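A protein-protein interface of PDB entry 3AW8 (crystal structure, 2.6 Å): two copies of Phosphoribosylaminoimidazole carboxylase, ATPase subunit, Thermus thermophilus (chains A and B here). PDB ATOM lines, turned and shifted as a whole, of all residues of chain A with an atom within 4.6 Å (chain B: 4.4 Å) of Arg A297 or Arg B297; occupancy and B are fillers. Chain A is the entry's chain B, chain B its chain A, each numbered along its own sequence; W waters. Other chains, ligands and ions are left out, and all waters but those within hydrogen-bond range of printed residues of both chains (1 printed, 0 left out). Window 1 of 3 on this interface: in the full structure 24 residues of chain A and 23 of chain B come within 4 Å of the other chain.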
ATOM      1  N   ILE A 271     -17.734 -28.172  37.243  1.00  0.00           N
ATOM      2  CA  ILE A 271     -18.030 -29.508  36.731  1.00  0.00           C
ATOM      3  C   ILE A 271     -18.624 -29.373  35.327  1.00  0.00           C
ATOM      4  O   ILE A 271     -18.235 -30.096  34.418  1.00  0.00           O
ATOM      5  CB  ILE A 271     -18.993 -30.274  37.654  1.00  0.00           C
ATOM      6  CG1 ILE A 271     -18.317 -30.548  39.002  1.00  0.00           C
ATOM      7  CG2 ILE A 271     -19.366 -31.595  37.025  1.00  0.00           C
ATOM      8  CD1 ILE A 271     -19.211 -31.238  40.016  1.00  0.00           C
ATOM      9  N   GLU A 272     -19.555 -28.444  35.140  1.00  0.00           N
ATOM     10  CA  GLU A 272     -20.115 -28.227  33.811  1.00  0.00           C
ATOM     11  C   GLU A 272     -19.919 -26.788  33.313  1.00  0.00           C
ATOM     12  O   GLU A 272     -20.125 -26.511  32.136  1.00  0.00           O
ATOM     13  CB  GLU A 272     -21.601 -28.622  33.747  1.00  0.00           C
ATOM     14  CG  GLU A 272     -22.466 -28.190  34.912  1.00  0.00           C
ATOM     15  CD  GLU A 272     -22.439 -29.181  36.064  1.00  0.00           C
ATOM     16  OE1 GLU A 272     -21.842 -28.865  37.118  1.00  0.00           O
ATOM     17  OE2 GLU A 272     -23.014 -30.281  35.914  1.00  0.00           O
ATOM     18  N   GLY A 273     -19.485 -25.888  34.194  1.00  0.00           N
ATOM     19  CA  GLY A 273     -19.271 -24.500  33.802  1.00  0.00           C
ATOM     20  C   GLY A 273     -17.865 -24.093  33.348  1.00  0.00           C
ATOM     21  O   GLY A 273     -17.603 -22.910  33.117  1.00  0.00           O
ATOM     22  N   ALA A 274     -16.951 -25.053  33.231  1.00  0.00           N
ATOM     23  CA  ALA A 274     -15.591 -24.765  32.779  1.00  0.00           C
ATOM     24  C   ALA A 274     -15.104 -25.953  31.959  1.00  0.00           C
ATOM     25  O   ALA A 274     -15.606 -27.069  32.104  1.00  0.00           O
ATOM     26  CB  ALA A 274     -14.664 -24.518  33.969  1.00  0.00           C
ATOM     27  N   GLU A 275     -14.124 -25.722  31.102  1.00  0.00           N
ATOM     28  CA  GLU A 275     -13.625 -26.785  30.255  1.00  0.00           C
ATOM     29  C   GLU A 275     -13.132 -27.978  31.061  1.00  0.00           C
ATOM     30  O   GLU A 275     -13.260 -29.127  30.630  1.00  0.00           O
ATOM     31  CB  GLU A 275     -12.508 -26.255  29.354  1.00  0.00           C
ATOM     32  CG  GLU A 275     -12.466 -26.931  27.993  1.00  0.00           C
ATOM     33  CD  GLU A 275     -13.824 -26.913  27.301  1.00  0.00           C
ATOM     34  OE1 GLU A 275     -14.459 -25.829  27.290  1.00  0.00           O
ATOM     35  OE2 GLU A 275     -14.251 -27.968  26.771  1.00  0.00           O
ATOM     36  N   ALA A 295     -10.993 -22.393  31.010  1.00  0.00           N
ATOM     37  CA  ALA A 295     -11.892 -21.421  30.401  1.00  0.00           C
ATOM     38  C   ALA A 295     -13.342 -21.686  30.785  1.00  0.00           C
ATOM     39  O   ALA A 295     -13.811 -22.815  30.722  1.00  0.00           O
ATOM     40  CB  ALA A 295     -11.742 -21.457  28.890  1.00  0.00           C
ATOM     41  N   PRO A 296     -14.073 -20.641  31.197  1.00  0.00           N
ATOM     42  CA  PRO A 296     -15.476 -20.800  31.583  1.00  0.00           C
ATOM     43  C   PRO A 296     -16.363 -21.143  30.395  1.00  0.00           C
ATOM     44  O   PRO A 296     -16.131 -20.678  29.280  1.00  0.00           O
ATOM     45  CB  PRO A 296     -15.824 -19.445  32.186  1.00  0.00           C
ATOM     46  CG  PRO A 296     -14.953 -18.512  31.425  1.00  0.00           C
ATOM     47  CD  PRO A 296     -13.639 -19.246  31.374  1.00  0.00           C
ATOM     48  N   ARG A 297     -17.373 -21.972  30.639  1.00  0.00           N
ATOM     49  CA  ARG A 297     -18.313 -22.383  29.604  1.00  0.00           C
ATOM     50  C   ARG A 297     -19.567 -21.575  29.886  1.00  0.00           C
ATOM     51  O   ARG A 297     -20.461 -22.031  30.604  1.00  0.00           O
ATOM     52  CB  ARG A 297     -18.602 -23.889  29.718  1.00  0.00           C
ATOM     53  CG  ARG A 297     -18.450 -24.655  28.409  1.00  0.00           C
ATOM     54  CD  ARG A 297     -17.547 -25.897  28.522  1.00  0.00           C
ATOM     55  NE  ARG A 297     -18.185 -27.023  29.204  1.00  0.00           N
ATOM     56  CZ  ARG A 297     -17.642 -28.235  29.334  1.00  0.00           C
ATOM     57  NH1 ARG A 297     -16.444 -28.489  28.822  1.00  0.00           N
ATOM     58  NH2 ARG A 297     -18.293 -29.192  29.989  1.00  0.00           N
ATOM     59  N   GLY A 298     -19.612 -20.358  29.346  1.00  0.00           N
ATOM     60  CA  GLY A 298     -20.755 -19.487  29.569  1.00  0.00           C
ATOM     61  C   GLY A 298     -20.736 -18.810  30.931  1.00  0.00           C
ATOM     62  O   GLY A 298     -19.744 -18.197  31.317  1.00  0.00           O
ATOM     63  N   GLN A 299     -21.841 -18.915  31.657  1.00  0.00           N
ATOM     64  CA  GLN A 299     -21.968 -18.321  32.985  1.00  0.00           C
ATOM     65  C   GLN A 299     -22.618 -19.315  33.933  1.00  0.00           C
ATOM     66  O   GLN A 299     -23.503 -20.071  33.541  1.00  0.00           O
ATOM     67  CB  GLN A 299     -22.821 -17.062  32.927  1.00  0.00           C
ATOM     68  CG  GLN A 299     -22.025 -15.788  32.838  1.00  0.00           C
ATOM     69  CD  GLN A 299     -22.833 -14.670  32.226  1.00  0.00           C
ATOM     70  OE1 GLN A 299     -23.141 -14.701  31.031  1.00  0.00           O
ATOM     71  NE2 GLN A 299     -23.197 -13.678  33.040  1.00  0.00           N
ATOM     72  N   HIS A 322     -28.145 -28.181  36.676  1.00  0.00           N
ATOM     73  CA  HIS A 322     -27.504 -29.484  36.885  1.00  0.00           C
ATOM     74  C   HIS A 322     -27.527 -29.856  38.359  1.00  0.00           C
ATOM     75  O   HIS A 322     -26.871 -29.224  39.181  1.00  0.00           O
ATOM     76  CB  HIS A 322     -26.072 -29.464  36.362  1.00  0.00           C
ATOM     77  CG  HIS A 322     -25.972 -29.169  34.897  1.00  0.00           C
ATOM     78  ND1 HIS A 322     -25.827 -27.890  34.402  1.00  0.00           N
ATOM     79  CD2 HIS A 322     -25.993 -29.990  33.819  1.00  0.00           C
ATOM     80  CE1 HIS A 322     -25.757 -27.936  33.083  1.00  0.00           C
ATOM     81  NE2 HIS A 322     -25.854 -29.198  32.704  1.00  0.00           N
ATOM     82  N   ARG A 342     -25.975 -23.208  34.462  1.00  0.00           N
ATOM     83  CA  ARG A 342     -25.120 -22.499  33.526  1.00  0.00           C
ATOM     84  C   ARG A 342     -25.859 -22.208  32.222  1.00  0.00           C
ATOM     85  O   ARG A 342     -26.388 -23.110  31.569  1.00  0.00           O
ATOM     86  CB  ARG A 342     -23.828 -23.279  33.254  1.00  0.00           C
ATOM     87  CG  ARG A 342     -23.953 -24.357  32.229  1.00  0.00           C
ATOM     88  CD  ARG A 342     -22.640 -24.554  31.522  1.00  0.00           C
ATOM     89  NE  ARG A 342     -22.856 -24.843  30.112  1.00  0.00           N
ATOM     90  CZ  ARG A 342     -23.395 -23.986  29.245  1.00  0.00           C
ATOM     91  NH1 ARG A 342     -23.554 -24.335  27.975  1.00  0.00           N
ATOM     92  NH2 ARG A 342     -23.771 -22.776  29.641  1.00  0.00           N
ATOM     93  N   GLU B 272     -19.941 -34.048  27.363  1.00  0.00           N
ATOM     94  CA  GLU B 272     -19.478 -32.670  27.499  1.00  0.00           C
ATOM     95  C   GLU B 272     -19.963 -31.775  26.354  1.00  0.00           C
ATOM     96  O   GLU B 272     -20.026 -30.560  26.509  1.00  0.00           O
ATOM     97  CB  GLU B 272     -17.955 -32.605  27.603  1.00  0.00           C
ATOM     98  CG  GLU B 272     -17.253 -33.662  26.814  1.00  0.00           C
ATOM     99  CD  GLU B 272     -16.928 -34.871  27.659  1.00  0.00           C
ATOM    100  OE1 GLU B 272     -17.158 -36.004  27.188  1.00  0.00           O
ATOM    101  OE2 GLU B 272     -16.435 -34.683  28.791  1.00  0.00           O
ATOM    102  N   GLY B 273     -20.337 -32.377  25.224  1.00  0.00           N
ATOM    103  CA  GLY B 273     -20.809 -31.603  24.083  1.00  0.00           C
ATOM    104  C   GLY B 273     -22.303 -31.278  23.982  1.00  0.00           C
ATOM    105  O   GLY B 273     -22.738 -30.667  23.003  1.00  0.00           O
ATOM    106  N   ALA B 274     -23.099 -31.692  24.963  1.00  0.00           N
ATOM    107  CA  ALA B 274     -24.533 -31.404  24.951  1.00  0.00           C
ATOM    108  C   ALA B 274     -24.908 -30.968  26.361  1.00  0.00           C
ATOM    109  O   ALA B 274     -24.224 -31.319  27.319  1.00  0.00           O
ATOM    110  CB  ALA B 274     -25.324 -32.636  24.544  1.00  0.00           C
ATOM    111  N   GLU B 275     -25.987 -30.211  26.506  1.00  0.00           N
ATOM    112  CA  GLU B 275     -26.359 -29.741  27.830  1.00  0.00           C
ATOM    113  C   GLU B 275     -26.681 -30.871  28.792  1.00  0.00           C
ATOM    114  O   GLU B 275     -26.541 -30.724  30.008  1.00  0.00           O
ATOM    115  CB  GLU B 275     -27.544 -28.772  27.751  1.00  0.00           C
ATOM    116  CG  GLU B 275     -27.637 -27.873  28.980  1.00  0.00           C
ATOM    117  CD  GLU B 275     -26.367 -27.053  29.194  1.00  0.00           C
ATOM    118  OE1 GLU B 275     -26.095 -26.632  30.345  1.00  0.00           O
ATOM    119  OE2 GLU B 275     -25.643 -26.822  28.198  1.00  0.00           O
ATOM    120  N   ALA B 295     -29.683 -29.468  23.823  1.00  0.00           N
ATOM    121  CA  ALA B 295     -28.953 -28.467  23.057  1.00  0.00           C
ATOM    122  C   ALA B 295     -27.444 -28.737  23.073  1.00  0.00           C
ATOM    123  O   ALA B 295     -26.870 -29.051  24.114  1.00  0.00           O
ATOM    124  CB  ALA B 295     -29.248 -27.080  23.609  1.00  0.00           C
ATOM    125  N   PRO B 296     -26.786 -28.632  21.909  1.00  0.00           N
ATOM    126  CA  PRO B 296     -25.342 -28.872  21.825  1.00  0.00           C
ATOM    127  C   PRO B 296     -24.493 -27.712  22.326  1.00  0.00           C
ATOM    128  O   PRO B 296     -24.897 -26.554  22.250  1.00  0.00           O
ATOM    129  CB  PRO B 296     -25.123 -29.128  20.338  1.00  0.00           C
ATOM    130  CG  PRO B 296     -26.139 -28.250  19.708  1.00  0.00           C
ATOM    131  CD  PRO B 296     -27.367 -28.475  20.566  1.00  0.00           C
ATOM    132  N   ARG B 297     -23.320 -28.041  22.857  1.00  0.00           N
ATOM    133  CA  ARG B 297     -22.380 -27.042  23.344  1.00  0.00           C
ATOM    134  C   ARG B 297     -21.289 -26.994  22.291  1.00  0.00           C
ATOM    135  O   ARG B 297     -20.359 -27.806  22.310  1.00  0.00           O
ATOM    136  CB  ARG B 297     -21.769 -27.458  24.684  1.00  0.00           C
ATOM    137  CG  ARG B 297     -22.713 -27.404  25.879  1.00  0.00           C
ATOM    138  CD  ARG B 297     -22.017 -27.964  27.109  1.00  0.00           C
ATOM    139  NE  ARG B 297     -22.888 -28.062  28.277  1.00  0.00           N
ATOM    140  CZ  ARG B 297     -22.608 -28.800  29.349  1.00  0.00           C
ATOM    141  NH1 ARG B 297     -23.448 -28.836  30.373  1.00  0.00           N
ATOM    142  NH2 ARG B 297     -21.489 -29.519  29.390  1.00  0.00           N
ATOM    143  N   GLY B 298     -21.423 -26.062  21.353  1.00  0.00           N
ATOM    144  CA  GLY B 298     -20.433 -25.940  20.301  1.00  0.00           C
ATOM    145  C   GLY B 298     -20.423 -27.128  19.363  1.00  0.00           C
ATOM    146  O   GLY B 298     -21.473 -27.569  18.898  1.00  0.00           O
ATOM    147  N   GLN B 299     -19.232 -27.645  19.087  1.00  0.00           N
ATOM    148  CA  GLN B 299     -19.063 -28.778  18.187  1.00  0.00           C
ATOM    149  C   GLN B 299     -18.201 -29.874  18.790  1.00  0.00           C
ATOM    150  O   GLN B 299     -17.203 -29.606  19.455  1.00  0.00           O
ATOM    151  CB  GLN B 299     -18.415 -28.322  16.889  1.00  0.00           C
ATOM    152  CG  GLN B 299     -19.335 -27.668  15.905  1.00  0.00           C
ATOM    153  CD  GLN B 299     -18.559 -27.169  14.714  1.00  0.00           C
ATOM    154  OE1 GLN B 299     -17.764 -26.234  14.833  1.00  0.00           O
ATOM    155  NE2 GLN B 299     -18.759 -27.803  13.558  1.00  0.00           N
ATOM    156  N   HIS B 322     -11.407 -34.389  25.851  1.00  0.00           N
ATOM    157  CA  HIS B 322     -11.846 -35.054  27.079  1.00  0.00           C
ATOM    158  C   HIS B 322     -11.644 -36.555  26.956  1.00  0.00           C
ATOM    159  O   HIS B 322     -12.333 -37.230  26.188  1.00  0.00           O
ATOM    160  CB  HIS B 322     -13.310 -34.741  27.375  1.00  0.00           C
ATOM    161  CG  HIS B 322     -13.576 -33.285  27.598  1.00  0.00           C
ATOM    162  ND1 HIS B 322     -13.890 -32.419  26.574  1.00  0.00           N
ATOM    163  CD2 HIS B 322     -13.562 -32.540  28.729  1.00  0.00           C
ATOM    164  CE1 HIS B 322     -14.064 -31.204  27.063  1.00  0.00           C
ATOM    165  NE2 HIS B 322     -13.871 -31.250  28.369  1.00  0.00           N
ATOM    166  N   ARG B 342     -14.334 -31.052  22.187  1.00  0.00           N
ATOM    167  CA  ARG B 342     -15.399 -30.068  22.100  1.00  0.00           C
ATOM    168  C   ARG B 342     -14.824 -28.663  21.958  1.00  0.00           C
ATOM    169  O   ARG B 342     -14.290 -28.101  22.913  1.00  0.00           O
ATOM    170  CB  ARG B 342     -16.277 -30.138  23.349  1.00  0.00           C
ATOM    171  CG  ARG B 342     -17.604 -29.427  23.213  1.00  0.00           C
ATOM    172  CD  ARG B 342     -18.130 -29.041  24.572  1.00  0.00           C
ATOM    173  NE  ARG B 342     -17.270 -28.037  25.183  1.00  0.00           N
ATOM    174  CZ  ARG B 342     -17.114 -26.802  24.713  1.00  0.00           C
ATOM    175  NH1 ARG B 342     -17.767 -26.416  23.624  1.00  0.00           N
ATOM    176  NH2 ARG B 342     -16.305 -25.947  25.326  1.00  0.00           N
HETATM  177  O   HOH W   1     -19.965 -31.363  31.315  1.00  0.00           O
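O of Glu B275 lies within hydrogen-bond range of NE2 of His A322 (3.2 Å). The side-chain carboxylate (OE2) of Glu B275 is in salt-bridge range of the guanidinium group (NH1) of Arg A342, at 3.3 Å. NE2 of His A322 sits at hydrogen-bond distance from NH1 of Arg B297, 3.4 Å away. O of Glu A275 sits at hydrogen-bond distance from NE2 of His B322 (3.2 Å). OE1 of Glu A275 is in salt-bridge range of NH2 of Arg B342, at 2.7 Å. The guanidinium group of Arg B297 lies close to the guanidinium group of Arg A297.
The backbone carbonyl oxygen (O) of Gly B273 sits at hydrogen-bond distance from the backbone NH (N) of Arg B297 (2.7 Å). N of Glu B275 sits at hydrogen-bond distance from O of Ala B295 (2.8 Å). NE of Arg B297 lies within salt-bridge range of OE2 of Glu B275 (3.0 Å). The guanidinium group of Arg B342 lies within hydrogen-bond range of the backbone carbonyl oxygen of Arg B297 (3.2 Å). O of Gly A273 lies within hydrogen-bond range of N of Arg A297 (2.7 Å). The side-chain carboxylate (OE2) of Glu A275 is in salt-bridge range of the guanidinium group (NH1) of Arg A297 (3.0 Å).
Arg B297 touches Glu A272 (NH1 to CB, 3.9 Å). NH1 of Arg A297 touches NE2 of His B322, at 3.8 Å. NH2 of Arg B342 touches CD of Arg A297, at 3.4 Å. NE of Arg B297 touches NE of Arg A342, 3.7 Å away.
Arg B297 touches just these residues of chain A: Glu A272 (3.9 Å), Arg A297 (3.3 Å), His A322 (3.4 Å) and Arg A342 (3.7 Å). Of the printed residues of chain B, Arg A342 touches Glu B275 and Arg B297. Of the printed residues of chain B, Glu A275 touches His B322 and Arg B342. The nearest printed residue of chain B that does not touch Glu A275 is Glu B272 (6.0 Å).
Of the 12 printed residues of chain A, 5 touch a printed residue of chain B. Hydrophobic or aromatic side chains of chain A that line the printed part of chain B: His A322. Among the printed residues, Asp or Glu carboxylates within 4 Å of a Lys or Arg side-chain nitrogen of the other chain: Glu A275 with Arg B342 and Arg A342 with Glu B275.
Glu A275 touches Arg B342, and with the chains exchanged Arg A342 touches Glu B275. Arg A297 touches its own counterpart, Arg B297. Arg A297 touches His B322, and with the chains exchanged His A322 touches Arg B297. Arg A297 touches Arg B342, and with the chains exchanged Arg A342 touches Arg B297. Positions printed for both chains: 272, 273, 274, 275, 295, 296, 297, 298, 299, 322 and 342. Of the 10 pairs that touch across the chains among the printed residues, 9 have their exchanged pair printed and touching as well.
Water W1 lies within hydrogen-bond range of the guanidinium group of Arg A297 and the guanidinium group of Arg B297.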
